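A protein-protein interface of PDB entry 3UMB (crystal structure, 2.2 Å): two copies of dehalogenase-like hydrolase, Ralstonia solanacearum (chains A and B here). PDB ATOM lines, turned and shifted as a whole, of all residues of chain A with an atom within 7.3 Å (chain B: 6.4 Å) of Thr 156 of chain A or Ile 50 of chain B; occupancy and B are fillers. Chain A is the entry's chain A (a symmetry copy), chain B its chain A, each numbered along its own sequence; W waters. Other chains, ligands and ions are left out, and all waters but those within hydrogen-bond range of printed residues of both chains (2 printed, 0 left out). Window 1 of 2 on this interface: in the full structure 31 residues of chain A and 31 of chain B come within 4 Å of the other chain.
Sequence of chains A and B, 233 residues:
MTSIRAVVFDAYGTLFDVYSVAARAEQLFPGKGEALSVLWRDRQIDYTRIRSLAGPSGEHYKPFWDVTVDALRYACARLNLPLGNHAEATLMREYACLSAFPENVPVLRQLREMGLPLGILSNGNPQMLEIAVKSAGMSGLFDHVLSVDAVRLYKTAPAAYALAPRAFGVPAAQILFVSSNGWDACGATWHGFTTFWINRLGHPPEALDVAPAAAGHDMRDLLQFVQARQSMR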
ATOM      1  N   THR A  48       6.680  -7.624 -10.242  1.00  0.00           N
ATOM      2  CA  THR A  48       6.848  -8.595  -9.127  1.00  0.00           C
ATOM      3  C   THR A  48       8.204  -8.383  -8.434  1.00  0.00           C
ATOM      4  O   THR A  48       8.289  -8.424  -7.231  1.00  0.00           O
ATOM      5  CB  THR A  48       6.777 -10.040  -9.610  1.00  0.00           C
ATOM      6  OG1 THR A  48       7.839 -10.290 -10.514  1.00  0.00           O
ATOM      7  CG2 THR A  48       5.431 -10.355 -10.287  1.00  0.00           C
ATOM      8  N   ARG A  49       9.260  -8.161  -9.214  1.00  0.00           N
ATOM      9  CA  ARG A  49      10.568  -7.893  -8.657  1.00  0.00           C
ATOM     10  C   ARG A  49      10.683  -6.561  -7.936  1.00  0.00           C
ATOM     11  O   ARG A  49      11.243  -6.493  -6.870  1.00  0.00           O
ATOM     12  CB  ARG A  49      11.596  -7.914  -9.747  1.00  0.00           C
ATOM     13  CG  ARG A  49      11.746  -9.281 -10.365  1.00  0.00           C
ATOM     14  CD  ARG A  49      12.571  -9.185 -11.584  1.00  0.00           C
ATOM     15  NE  ARG A  49      12.813 -10.483 -12.183  1.00  0.00           N
ATOM     16  CZ  ARG A  49      13.354 -10.647 -13.385  1.00  0.00           C
ATOM     17  NH1 ARG A  49      13.694  -9.584 -14.151  1.00  0.00           N
ATOM     18  NH2 ARG A  49      13.531 -11.872 -13.846  1.00  0.00           N
ATOM     19  N   SER A  52       8.924  -7.045  -4.539  1.00  0.00           N
ATOM     20  CA  SER A  52       9.492  -7.948  -3.538  1.00  0.00           C
ATOM     21  C   SER A  52      10.838  -7.417  -3.060  1.00  0.00           C
ATOM     22  O   SER A  52      11.170  -7.591  -1.878  1.00  0.00           O
ATOM     23  CB  SER A  52       9.573  -9.391  -4.092  1.00  0.00           C
ATOM     24  OG  SER A  52       8.236  -9.964  -4.189  1.00  0.00           O
ATOM     25  N   LEU A  53      11.594  -6.781  -3.975  1.00  0.00           N
ATOM     26  CA  LEU A  53      12.851  -6.125  -3.661  1.00  0.00           C
ATOM     27  C   LEU A  53      12.627  -4.977  -2.724  1.00  0.00           C
ATOM     28  O   LEU A  53      13.456  -4.803  -1.841  1.00  0.00           O
ATOM     29  CB  LEU A  53      13.631  -5.674  -4.930  1.00  0.00           C
ATOM     30  CG  LEU A  53      15.160  -5.397  -4.863  1.00  0.00           C
ATOM     31  CD1 LEU A  53      15.899  -6.441  -4.050  1.00  0.00           C
ATOM     32  CD2 LEU A  53      15.808  -5.333  -6.302  1.00  0.00           C
ATOM     33  N   ASN A 123       4.527 -18.179  -9.495  1.00  0.00           N
ATOM     34  CA  ASN A 123       4.323 -16.805  -9.044  1.00  0.00           C
ATOM     35  C   ASN A 123       2.797 -16.619  -8.959  1.00  0.00           C
ATOM     36  O   ASN A 123       2.266 -15.773  -8.214  1.00  0.00           O
ATOM     37  CB  ASN A 123       4.981 -15.795 -10.027  1.00  0.00           C
ATOM     38  CG  ASN A 123       6.457 -15.460  -9.689  1.00  0.00           C
ATOM     39  OD1 ASN A 123       6.969 -15.732  -8.597  1.00  0.00           O
ATOM     40  ND2 ASN A 123       7.140 -14.839 -10.648  1.00  0.00           N
ATOM     41  N   LEU A 153       6.020 -13.160  -1.391  1.00  0.00           N
ATOM     42  CA  LEU A 153       7.288 -12.761  -2.018  1.00  0.00           C
ATOM     43  C   LEU A 153       7.486 -13.547  -3.317  1.00  0.00           C
ATOM     44  O   LEU A 153       7.275 -14.807  -3.352  1.00  0.00           O
ATOM     45  CB  LEU A 153       8.475 -13.037  -1.093  1.00  0.00           C
ATOM     46  CG  LEU A 153       8.617 -12.138   0.156  1.00  0.00           C
ATOM     47  CD1 LEU A 153       9.438 -12.849   1.173  1.00  0.00           C
ATOM     48  CD2 LEU A 153       9.216 -10.717  -0.133  1.00  0.00           C
ATOM     49  N   TYR A 154       7.892 -12.847  -4.365  1.00  0.00           N
ATOM     50  CA  TYR A 154       8.054 -13.473  -5.678  1.00  0.00           C
ATOM     51  C   TYR A 154       9.450 -14.024  -5.839  1.00  0.00           C
ATOM     52  O   TYR A 154      10.398 -13.549  -5.226  1.00  0.00           O
ATOM     53  CB  TYR A 154       7.769 -12.446  -6.758  1.00  0.00           C
ATOM     54  CG  TYR A 154       6.318 -12.128  -6.879  1.00  0.00           C
ATOM     55  CD1 TYR A 154       5.810 -10.967  -6.380  1.00  0.00           C
ATOM     56  CD2 TYR A 154       5.433 -13.020  -7.501  1.00  0.00           C
ATOM     57  CE1 TYR A 154       4.443 -10.677  -6.467  1.00  0.00           C
ATOM     58  CE2 TYR A 154       4.046 -12.756  -7.568  1.00  0.00           C
ATOM     59  CZ  TYR A 154       3.568 -11.556  -7.094  1.00  0.00           C
ATOM     60  OH  TYR A 154       2.206 -11.237  -7.191  1.00  0.00           O
ATOM     61  N   LYS A 155       9.597 -15.031  -6.680  1.00  0.00           N
ATOM     62  CA  LYS A 155      10.913 -15.420  -7.164  1.00  0.00           C
ATOM     63  C   LYS A 155      11.585 -14.180  -7.669  1.00  0.00           C
ATOM     64  O   LYS A 155      10.916 -13.338  -8.293  1.00  0.00           O
ATOM     65  CB  LYS A 155      10.823 -16.392  -8.339  1.00  0.00           C
ATOM     66  CG  LYS A 155      10.118 -17.715  -8.018  1.00  0.00           C
ATOM     67  CD  LYS A 155       9.493 -18.263  -9.303  1.00  0.00           C
ATOM     68  CE  LYS A 155       9.262 -19.761  -9.303  1.00  0.00           C
ATOM     69  NZ  LYS A 155       8.583 -20.164 -10.625  1.00  0.00           N
ATOM     70  N   THR A 156      12.896 -14.054  -7.479  1.00  0.00           N
ATOM     71  CA  THR A 156      13.798 -15.129  -7.009  1.00  0.00           C
ATOM     72  C   THR A 156      14.018 -15.223  -5.487  1.00  0.00           C
ATOM     73  O   THR A 156      15.018 -15.780  -5.048  1.00  0.00           O
ATOM     74  CB  THR A 156      15.156 -14.924  -7.639  1.00  0.00           C
ATOM     75  OG1 THR A 156      15.468 -13.539  -7.564  1.00  0.00           O
ATOM     76  CG2 THR A 156      15.142 -15.311  -9.150  1.00  0.00           C
ATOM     77  N   ALA A 157      13.105 -14.657  -4.697  1.00  0.00           N
ATOM     78  CA  ALA A 157      13.209 -14.599  -3.258  1.00  0.00           C
ATOM     79  C   ALA A 157      13.375 -15.982  -2.632  1.00  0.00           C
ATOM     80  O   ALA A 157      12.623 -16.878  -2.994  1.00  0.00           O
ATOM     81  CB  ALA A 157      11.893 -13.906  -2.700  1.00  0.00           C
ATOM     82  N   PRO A 158      14.348 -16.167  -1.698  1.00  0.00           N
ATOM     83  CA  PRO A 158      14.543 -17.508  -1.086  1.00  0.00           C
ATOM     84  C   PRO A 158      13.250 -18.135  -0.525  1.00  0.00           C
ATOM     85  O   PRO A 158      13.062 -19.336  -0.626  1.00  0.00           O
ATOM     86  CB  PRO A 158      15.525 -17.260   0.058  1.00  0.00           C
ATOM     87  CG  PRO A 158      16.360 -16.088  -0.392  1.00  0.00           C
ATOM     88  CD  PRO A 158      15.484 -15.268  -1.386  1.00  0.00           C
ATOM     89  N   ALA A 159      12.377 -17.293   0.038  1.00  0.00           N
ATOM     90  CA  ALA A 159      11.178 -17.782   0.722  1.00  0.00           C
ATOM     91  C   ALA A 159      10.253 -18.448  -0.306  1.00  0.00           C
ATOM     92  O   ALA A 159       9.474 -19.329   0.070  1.00  0.00           O
ATOM     93  CB  ALA A 159      10.431 -16.640   1.450  1.00  0.00           C
ATOM     94  N   ALA A 160      10.310 -17.989  -1.563  1.00  0.00           N
ATOM     95  CA  ALA A 160       9.502 -18.585  -2.661  1.00  0.00           C
ATOM     96  C   ALA A 160      10.056 -19.934  -3.043  1.00  0.00           C
ATOM     97  O   ALA A 160       9.315 -20.891  -3.115  1.00  0.00           O
ATOM     98  CB  ALA A 160       9.453 -17.693  -3.891  1.00  0.00           C
ATOM     99  N   TYR A 161      11.360 -20.015  -3.284  1.00  0.00           N
ATOM    100  CA  TYR A 161      11.999 -21.297  -3.613  1.00  0.00           C
ATOM    101  C   TYR A 161      11.808 -22.298  -2.449  1.00  0.00           C
ATOM    102  O   TYR A 161      11.444 -23.476  -2.663  1.00  0.00           O
ATOM    103  CB  TYR A 161      13.478 -21.122  -3.990  1.00  0.00           C
ATOM    104  CG  TYR A 161      13.690 -20.432  -5.342  1.00  0.00           C
ATOM    105  CD1 TYR A 161      13.128 -20.960  -6.531  1.00  0.00           C
ATOM    106  CD2 TYR A 161      14.459 -19.288  -5.442  1.00  0.00           C
ATOM    107  CE1 TYR A 161      13.290 -20.319  -7.786  1.00  0.00           C
ATOM    108  CE2 TYR A 161      14.644 -18.634  -6.699  1.00  0.00           C
ATOM    109  CZ  TYR A 161      14.053 -19.160  -7.863  1.00  0.00           C
ATOM    110  OH  TYR A 161      14.259 -18.520  -9.074  1.00  0.00           O
ATOM    111  N   GLY A 182      15.068 -18.679 -18.048  1.00  0.00           N
ATOM    112  CA  GLY A 182      16.481 -18.793 -17.691  1.00  0.00           C
ATOM    113  C   GLY A 182      16.801 -18.204 -16.336  1.00  0.00           C
ATOM    114  O   GLY A 182      17.548 -18.807 -15.567  1.00  0.00           O
ATOM    115  N   TRP A 183      16.222 -17.048 -16.018  1.00  0.00           N
ATOM    116  CA  TRP A 183      16.522 -16.405 -14.736  1.00  0.00           C
ATOM    117  C   TRP A 183      16.100 -17.321 -13.581  1.00  0.00           C
ATOM    118  O   TRP A 183      16.763 -17.407 -12.554  1.00  0.00           O
ATOM    119  CB  TRP A 183      15.882 -15.012 -14.625  1.00  0.00           C
ATOM    120  CG  TRP A 183      14.376 -14.957 -14.813  1.00  0.00           C
ATOM    121  CD1 TRP A 183      13.719 -14.668 -15.976  1.00  0.00           C
ATOM    122  CD2 TRP A 183      13.360 -15.190 -13.825  1.00  0.00           C
ATOM    123  NE1 TRP A 183      12.352 -14.776 -15.789  1.00  0.00           N
ATOM    124  CE2 TRP A 183      12.111 -15.055 -14.469  1.00  0.00           C
ATOM    125  CE3 TRP A 183      13.386 -15.526 -12.468  1.00  0.00           C
ATOM    126  CZ2 TRP A 183      10.884 -15.195 -13.789  1.00  0.00           C
ATOM    127  CZ3 TRP A 183      12.164 -15.720 -11.789  1.00  0.00           C
ATOM    128  CH2 TRP A 183      10.929 -15.554 -12.464  1.00  0.00           C
ATOM    129  N   ASP A 184      14.990 -18.015 -13.756  1.00  0.00           N
ATOM    130  CA  ASP A 184      14.437 -18.863 -12.723  1.00  0.00           C
ATOM    131  C   ASP A 184      15.248 -20.154 -12.598  1.00  0.00           C
ATOM    132  O   ASP A 184      15.535 -20.585 -11.478  1.00  0.00           O
ATOM    133  CB  ASP A 184      12.976 -19.145 -13.057  1.00  0.00           C
ATOM    134  CG  ASP A 184      12.171 -19.663 -11.877  1.00  0.00           C
ATOM    135  OD1 ASP A 184      12.647 -19.665 -10.703  1.00  0.00           O
ATOM    136  OD2 ASP A 184      11.025 -20.053 -12.162  1.00  0.00           O
ATOM    137  N   ALA A 185      15.684 -20.749 -13.711  1.00  0.00           N
ATOM    138  CA  ALA A 185      16.572 -21.965 -13.605  1.00  0.00           C
ATOM    139  C   ALA A 185      17.789 -21.591 -12.804  1.00  0.00           C
ATOM    140  O   ALA A 185      18.254 -22.353 -11.940  1.00  0.00           O
ATOM    141  CB  ALA A 185      16.994 -22.522 -14.975  1.00  0.00           C
ATOM    142  N   CYS A 186      18.300 -20.403 -13.076  1.00  0.00           N
ATOM    143  CA  CYS A 186      19.516 -19.902 -12.427  1.00  0.00           C
ATOM    144  C   CYS A 186      19.298 -19.591 -10.942  1.00  0.00           C
ATOM    145  O   CYS A 186      20.146 -19.884 -10.095  1.00  0.00           O
ATOM    146  CB  CYS A 186      19.966 -18.630 -13.144  1.00  0.00           C
ATOM    147  SG  CYS A 186      20.779 -18.939 -14.756  1.00  0.00           S
ATOM    148  N   GLY A 187      18.165 -18.963 -10.638  1.00  0.00           N
ATOM    149  CA  GLY A 187      17.827 -18.662  -9.247  1.00  0.00           C
ATOM    150  C   GLY A 187      17.650 -19.958  -8.458  1.00  0.00           C
ATOM    151  O   GLY A 187      18.063 -20.042  -7.281  1.00  0.00           O
ATOM    152  N   ALA A 188      17.028 -20.965  -9.090  1.00  0.00           N
ATOM    153  CA  ALA A 188      16.812 -22.250  -8.430  1.00  0.00           C
ATOM    154  C   ALA A 188      18.104 -22.978  -8.177  1.00  0.00           C
ATOM    155  O   ALA A 188      18.252 -23.622  -7.151  1.00  0.00           O
ATOM    156  CB  ALA A 188      15.875 -23.090  -9.199  1.00  0.00           C
ATOM    157  N   TRP A 190      20.956 -21.559  -7.549  1.00  0.00           N
ATOM    158  CA  TRP A 190      21.523 -20.856  -6.382  1.00  0.00           C
ATOM    159  C   TRP A 190      20.882 -21.409  -5.108  1.00  0.00           C
ATOM    160  O   TRP A 190      21.516 -21.605  -4.124  1.00  0.00           O
ATOM    161  CB  TRP A 190      21.223 -19.324  -6.447  1.00  0.00           C
ATOM    162  CG  TRP A 190      22.142 -18.471  -7.293  1.00  0.00           C
ATOM    163  CD1 TRP A 190      23.450 -18.727  -7.628  1.00  0.00           C
ATOM    164  CD2 TRP A 190      21.841 -17.182  -7.862  1.00  0.00           C
ATOM    165  NE1 TRP A 190      23.954 -17.713  -8.407  1.00  0.00           N
ATOM    166  CE2 TRP A 190      22.995 -16.742  -8.541  1.00  0.00           C
ATOM    167  CE3 TRP A 190      20.696 -16.374  -7.889  1.00  0.00           C
ATOM    168  CZ2 TRP A 190      23.031 -15.548  -9.232  1.00  0.00           C
ATOM    169  CZ3 TRP A 190      20.739 -15.186  -8.581  1.00  0.00           C
ATOM    170  CH2 TRP A 190      21.897 -14.783  -9.238  1.00  0.00           C
ATOM    171  N   HIS A 191      19.602 -21.643  -5.113  1.00  0.00           N
ATOM    172  CA  HIS A 191      18.969 -22.142  -3.894  1.00  0.00           C
ATOM    173  C   HIS A 191      19.415 -23.567  -3.530  1.00  0.00           C
ATOM    174  O   HIS A 191      19.312 -23.978  -2.388  1.00  0.00           O
ATOM    175  CB  HIS A 191      17.463 -22.085  -4.049  1.00  0.00           C
ATOM    176  CG  HIS A 191      16.699 -22.362  -2.785  1.00  0.00           C
ATOM    177  ND1 HIS A 191      16.650 -21.470  -1.736  1.00  0.00           N
ATOM    178  CD2 HIS A 191      15.942 -23.419  -2.414  1.00  0.00           C
ATOM    179  CE1 HIS A 191      15.876 -21.959  -0.783  1.00  0.00           C
ATOM    180  NE2 HIS A 191      15.438 -23.143  -1.166  1.00  0.00           N
ATOM    181  N   GLU A 206      21.715 -17.054 -19.315  1.00  0.00           N
ATOM    182  CA  GLU A 206      21.832 -15.781 -18.619  1.00  0.00           C
ATOM    183  C   GLU A 206      23.245 -15.656 -18.078  1.00  0.00           C
ATOM    184  O   GLU A 206      23.838 -16.628 -17.645  1.00  0.00           O
ATOM    185  CB  GLU A 206      20.817 -15.664 -17.485  1.00  0.00           C
ATOM    186  CG  GLU A 206      19.387 -15.656 -17.932  1.00  0.00           C
ATOM    187  CD  GLU A 206      18.982 -14.453 -18.798  1.00  0.00           C
ATOM    188  OE1 GLU A 206      19.727 -13.492 -19.006  1.00  0.00           O
ATOM    189  OE2 GLU A 206      17.859 -14.458 -19.281  1.00  0.00           O
ATOM    190  N   LEU A 208      24.778 -14.937 -15.353  1.00  0.00           N
ATOM    191  CA  LEU A 208      24.586 -14.855 -13.894  1.00  0.00           C
ATOM    192  C   LEU A 208      25.661 -15.617 -13.114  1.00  0.00           C
ATOM    193  O   LEU A 208      25.539 -15.760 -11.910  1.00  0.00           O
ATOM    194  CB  LEU A 208      23.175 -15.319 -13.483  1.00  0.00           C
ATOM    195  CG  LEU A 208      21.993 -14.373 -13.849  1.00  0.00           C
ATOM    196  CD1 LEU A 208      20.643 -15.098 -13.725  1.00  0.00           C
ATOM    197  CD2 LEU A 208      21.937 -13.100 -13.076  1.00  0.00           C
ATOM    198  N   ILE B  45      19.474  -3.997 -15.703  1.00  0.00           N
ATOM    199  CA  ILE B  45      18.568  -3.823 -14.623  1.00  0.00           C
ATOM    200  C   ILE B  45      17.972  -5.154 -14.165  1.00  0.00           C
ATOM    201  O   ILE B  45      17.928  -5.415 -12.999  1.00  0.00           O
ATOM    202  CB  ILE B  45      17.562  -2.747 -14.979  1.00  0.00           C
ATOM    203  CG1 ILE B  45      18.276  -1.401 -14.995  1.00  0.00           C
ATOM    204  CG2 ILE B  45      16.431  -2.666 -13.951  1.00  0.00           C
ATOM    205  CD1 ILE B  45      18.895  -1.009 -13.586  1.00  0.00           C
ATOM    206  N   ASP B  46      17.560  -6.013 -15.080  1.00  0.00           N
ATOM    207  CA  ASP B  46      17.042  -7.297 -14.699  1.00  0.00           C
ATOM    208  C   ASP B  46      18.024  -8.004 -13.782  1.00  0.00           C
ATOM    209  O   ASP B  46      17.607  -8.579 -12.779  1.00  0.00           O
ATOM    210  CB  ASP B  46      16.826  -8.171 -15.918  1.00  0.00           C
ATOM    211  CG  ASP B  46      15.613  -7.774 -16.707  1.00  0.00           C
ATOM    212  OD1 ASP B  46      14.894  -6.848 -16.233  1.00  0.00           O
ATOM    213  OD2 ASP B  46      15.424  -8.385 -17.802  1.00  0.00           O
ATOM    214  N   TYR B  47      19.322  -7.984 -14.142  1.00  0.00           N
ATOM    215  CA  TYR B  47      20.343  -8.697 -13.388  1.00  0.00           C
ATOM    216  C   TYR B  47      20.556  -8.124 -12.001  1.00  0.00           C
ATOM    217  O   TYR B  47      20.757  -8.882 -11.075  1.00  0.00           O
ATOM    218  CB  TYR B  47      21.673  -8.795 -14.150  1.00  0.00           C
ATOM    219  CG  TYR B  47      21.678  -9.722 -15.379  1.00  0.00           C
ATOM    220  CD1 TYR B  47      20.599 -10.591 -15.674  1.00  0.00           C
ATOM    221  CD2 TYR B  47      22.779  -9.784 -16.218  1.00  0.00           C
ATOM    222  CE1 TYR B  47      20.615 -11.444 -16.823  1.00  0.00           C
ATOM    223  CE2 TYR B  47      22.804 -10.639 -17.366  1.00  0.00           C
ATOM    224  CZ  TYR B  47      21.733 -11.465 -17.640  1.00  0.00           C
ATOM    225  OH  TYR B  47      21.791 -12.303 -18.735  1.00  0.00           O
ATOM    226  N   THR B  48      20.469  -6.809 -11.824  1.00  0.00           N
ATOM    227  CA  THR B  48      20.609  -6.239 -10.458  1.00  0.00           C
ATOM    228  C   THR B  48      19.450  -6.707  -9.561  1.00  0.00           C
ATOM    229  O   THR B  48      19.657  -7.044  -8.421  1.00  0.00           O
ATOM    230  CB  THR B  48      20.618  -4.714 -10.471  1.00  0.00           C
ATOM    231  OG1 THR B  48      19.382  -4.237 -10.972  1.00  0.00           O
ATOM    232  CG2 THR B  48      21.775  -4.153 -11.318  1.00  0.00           C
ATOM    233  N   ARG B  49      18.231  -6.717 -10.096  1.00  0.00           N
ATOM    234  CA  ARG B  49      17.085  -7.195  -9.354  1.00  0.00           C
ATOM    235  C   ARG B  49      17.094  -8.688  -9.076  1.00  0.00           C
ATOM    236  O   ARG B  49      16.803  -9.105  -7.982  1.00  0.00           O
ATOM    237  CB  ARG B  49      15.828  -6.877 -10.106  1.00  0.00           C
ATOM    238  CG  ARG B  49      15.588  -5.392 -10.215  1.00  0.00           C
ATOM    239  CD  ARG B  49      14.492  -5.138 -11.170  1.00  0.00           C
ATOM    240  NE  ARG B  49      14.165  -3.729 -11.261  1.00  0.00           N
ATOM    241  CZ  ARG B  49      13.359  -3.221 -12.187  1.00  0.00           C
ATOM    242  NH1 ARG B  49      12.805  -4.007 -13.140  1.00  0.00           N
ATOM    243  NH2 ARG B  49      13.124  -1.921 -12.190  1.00  0.00           N
ATOM    244  N   ILE B  50      17.419  -9.493 -10.077  1.00  0.00           N
ATOM    245  CA  ILE B  50      17.470 -10.928  -9.899  1.00  0.00           C
ATOM    246  C   ILE B  50      18.424 -11.251  -8.749  1.00  0.00           C
ATOM    247  O   ILE B  50      18.086 -12.018  -7.837  1.00  0.00           O
ATOM    248  CB  ILE B  50      17.943 -11.642 -11.206  1.00  0.00           C
ATOM    249  CG1 ILE B  50      16.873 -11.578 -12.261  1.00  0.00           C
ATOM    250  CG2 ILE B  50      18.360 -13.128 -10.932  1.00  0.00           C
ATOM    251  CD1 ILE B  50      17.349 -12.060 -13.600  1.00  0.00           C
ATOM    252  N   ARG B  51      19.622 -10.683  -8.811  1.00  0.00           N
ATOM    253  CA  ARG B  51      20.629 -10.841  -7.757  1.00  0.00           C
ATOM    254  C   ARG B  51      20.210 -10.400  -6.356  1.00  0.00           C
ATOM    255  O   ARG B  51      20.464 -11.119  -5.381  1.00  0.00           O
ATOM    256  CB  ARG B  51      21.907 -10.077  -8.142  1.00  0.00           C
ATOM    257  CG  ARG B  51      22.633 -10.712  -9.347  1.00  0.00           C
ATOM    258  CD  ARG B  51      23.955 -10.011  -9.711  1.00  0.00           C
ATOM    259  NE  ARG B  51      24.727 -10.757 -10.705  1.00  0.00           N
ATOM    260  CZ  ARG B  51      25.461 -11.833 -10.451  1.00  0.00           C
ATOM    261  NH1 ARG B  51      25.581 -12.286  -9.212  1.00  0.00           N
ATOM    262  NH2 ARG B  51      26.099 -12.452 -11.445  1.00  0.00           N
ATOM    263  N   SER B  52      19.630  -9.214  -6.219  1.00  0.00           N
ATOM    264  CA  SER B  52      19.352  -8.688  -4.883  1.00  0.00           C
ATOM    265  C   SER B  52      18.140  -9.392  -4.286  1.00  0.00           C
ATOM    266  O   SER B  52      18.107  -9.606  -3.065  1.00  0.00           O
ATOM    267  CB  SER B  52      19.198  -7.148  -4.926  1.00  0.00           C
ATOM    268  OG  SER B  52      20.494  -6.522  -5.157  1.00  0.00           O
ATOM    269  N   LEU B  53      17.163  -9.741  -5.145  1.00  0.00           N
ATOM    270  CA  LEU B  53      15.994 -10.510  -4.759  1.00  0.00           C
ATOM    271  C   LEU B  53      16.391 -11.882  -4.306  1.00  0.00           C
ATOM    272  O   LEU B  53      15.790 -12.354  -3.349  1.00  0.00           O
ATOM    273  CB  LEU B  53      14.917 -10.575  -5.881  1.00  0.00           C
ATOM    274  CG  LEU B  53      13.439 -10.918  -5.540  1.00  0.00           C
ATOM    275  CD1 LEU B  53      12.956 -10.208  -4.292  1.00  0.00           C
ATOM    276  CD2 LEU B  53      12.464 -10.559  -6.730  1.00  0.00           C
ATOM    277  N   ALA B  54      17.435 -12.469  -4.909  1.00  0.00           N
ATOM    278  CA  ALA B  54      17.886 -13.847  -4.628  1.00  0.00           C
ATOM    279  C   ALA B  54      18.692 -13.955  -3.347  1.00  0.00           C
ATOM    280  O   ALA B  54      18.798 -15.052  -2.792  1.00  0.00           O
ATOM    281  CB  ALA B  54      18.779 -14.460  -5.801  1.00  0.00           C
ATOM    282  N   GLY B  55      19.341 -12.847  -2.966  1.00  0.00           N
ATOM    283  CA  GLY B  55      20.160 -12.772  -1.798  1.00  0.00           C
ATOM    284  C   GLY B  55      19.874 -11.485  -1.096  1.00  0.00           C
ATOM    285  O   GLY B  55      20.551 -10.496  -1.326  1.00  0.00           O
ATOM    286  N   HIS B  60      24.328 -12.573  -3.518  1.00  0.00           N
ATOM    287  CA  HIS B  60      24.618 -12.649  -4.945  1.00  0.00           C
ATOM    288  C   HIS B  60      24.998 -11.317  -5.526  1.00  0.00           C
ATOM    289  O   HIS B  60      24.918 -11.130  -6.716  1.00  0.00           O
ATOM    290  CB  HIS B  60      23.464 -13.317  -5.704  1.00  0.00           C
ATOM    291  CG  HIS B  60      23.185 -14.704  -5.231  1.00  0.00           C
ATOM    292  ND1 HIS B  60      24.050 -15.759  -5.453  1.00  0.00           N
ATOM    293  CD2 HIS B  60      22.152 -15.213  -4.517  1.00  0.00           C
ATOM    294  CE1 HIS B  60      23.558 -16.854  -4.899  1.00  0.00           C
ATOM    295  NE2 HIS B  60      22.397 -16.555  -4.340  1.00  0.00           N
HETATM  296  O   HOH W   1      13.197  -6.720 -14.085  1.00  0.00           O
HETATM  297  O   HOH W   2      17.080 -16.875  -3.589  1.00  0.00           O
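OH of Tyr 47 of chain B sits close to OE1 of Glu 206 of chain A (2.4 Å).
The backbone NH (N) of Ala 54 of chain B is in hydrogen-bond range of the side-chain hydroxyl (OG1) of Thr 156 of chain A (3.5 Å).
O of Leu 208 of chain A is in hydrogen-bond range of NH2 of Arg 51 of chain B (3.4 Å).
The backbone carbonyl oxygen of Ile 50 of chain B sits at hydrogen-bond distance from the side-chain hydroxyl of Thr 156 of chain A.
OD1 of Asp 46 of chain B lies within salt-bridge range of NH1 of Arg 49 of chain A, at 3.6 Å.
The side-chain hydroxyl (OG) of Ser 52 of chain A lies within hydrogen-bond range of the backbone carbonyl oxygen (O) of Thr 48 of chain A, 3.4 Å away.
NH1 of Arg 51 of chain B sits at hydrogen-bond distance from O of His 60 of chain B (2.8 Å).
The backbone NH (N) of Lys 155 of chain A is in hydrogen-bond range of the side-chain amide oxygen (OD1) of Asn 123 of chain A.
Among the printed residues, merely in contact across the chains: Arg 49 of chain A with Ile 50 of chain B (3.7 Å), Arg 49 of chain A with Leu 53 of chain B (3.8 Å), Ser 52 of chain A with Leu 53 of chain B (3.5 Å), Leu 53 of chain A with Arg 49 of chain B (3.8 Å), Leu 53 of chain A with Ser 52 of chain B (3.5 Å), Leu 53 of chain A with Leu 53 of chain B (3.7 Å), Tyr 154 of chain A with Leu 53 of chain B (3.9 Å), Lys 155 of chain A with Leu 53 of chain B (3.5 Å), Thr 156 of chain A with Leu 53 of chain B (3.5 Å), Ala 157 of chain A with Leu 53 of chain B (3.4 Å), Pro 158 of chain A with Leu 53 of chain B (3.5 Å), Pro 158 of chain A with Ala 54 of chain B (3.6 Å), Trp 183 of chain A with Ile 50 of chain B (3.5 Å), Trp 190 of chain A with Ile 50 of chain B (3.9 Å), Trp 190 of chain A with Ala 54 of chain B (3.4 Å), Trp 190 of chain A with His 60 of chain B (3.2 Å) and Leu 208 of chain A with Tyr 47 of chain B (3.9 Å).
Printed residues of chain B within 4 Å of Thr 156 of chain A: Ile 50, Leu 53 and Ala 54.
Printed residues of chain A within 4 Å of Ile 50 of chain B: Arg 49, Thr 156, Trp 183 and Trp 190.
Of the printed residues of chain B, Tyr 154 of chain A touches Leu 53.
Printed residues of chain B within 4 Å of Leu 208 of chain A: Tyr 47 (3.9 Å) and Arg 51 (3.4 Å).
The nearest residue of chain B that does not touch Thr 156 of chain A is Arg 49 of chain B (4.6 Å).
The nearest residue of chain A that does not touch Ile 50 of chain B is Leu 208 of chain A (4.1 Å).
The nearest printed residue of chain A that does not touch Asp 46 of chain B is Leu 208 of chain A (6.3 Å).
Printed residues of chain B that touch a printed residue of chain A: Asp 46, Tyr 47, Arg 49, Ile 50, Arg 51, Ser 52, Leu 53, Ala 54 and His 60.
Among the printed residues, 22 pairs touch across the chains.
Arg 49 of chain A touches Leu 53 of chain B, and with the chains exchanged Leu 53 of chain A touches Arg 49 of chain B.
Ser 52 of chain A touches Leu 53 of chain B, and with the chains exchanged Leu 53 of chain A touches Ser 52 of chain B.
Leu 53 of chain A touches its own counterpart, Leu 53 of chain B.
Positions printed for both chains: 48, 49, 52 and 53.
Water W2 bridges the backbone carbonyl oxygen of Ala 54 of chain B (2.6 Å) and the backbone carbonyl oxygen of Thr 156 of chain A (2.8 Å).
Water W1 lies within hydrogen-bond range of OD1 of Asp 46 of chain B (2.7 Å), NH1 of Arg 49 of chain B (2.9 Å) and NH1 of Arg 49 of chain A (2.9 Å).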
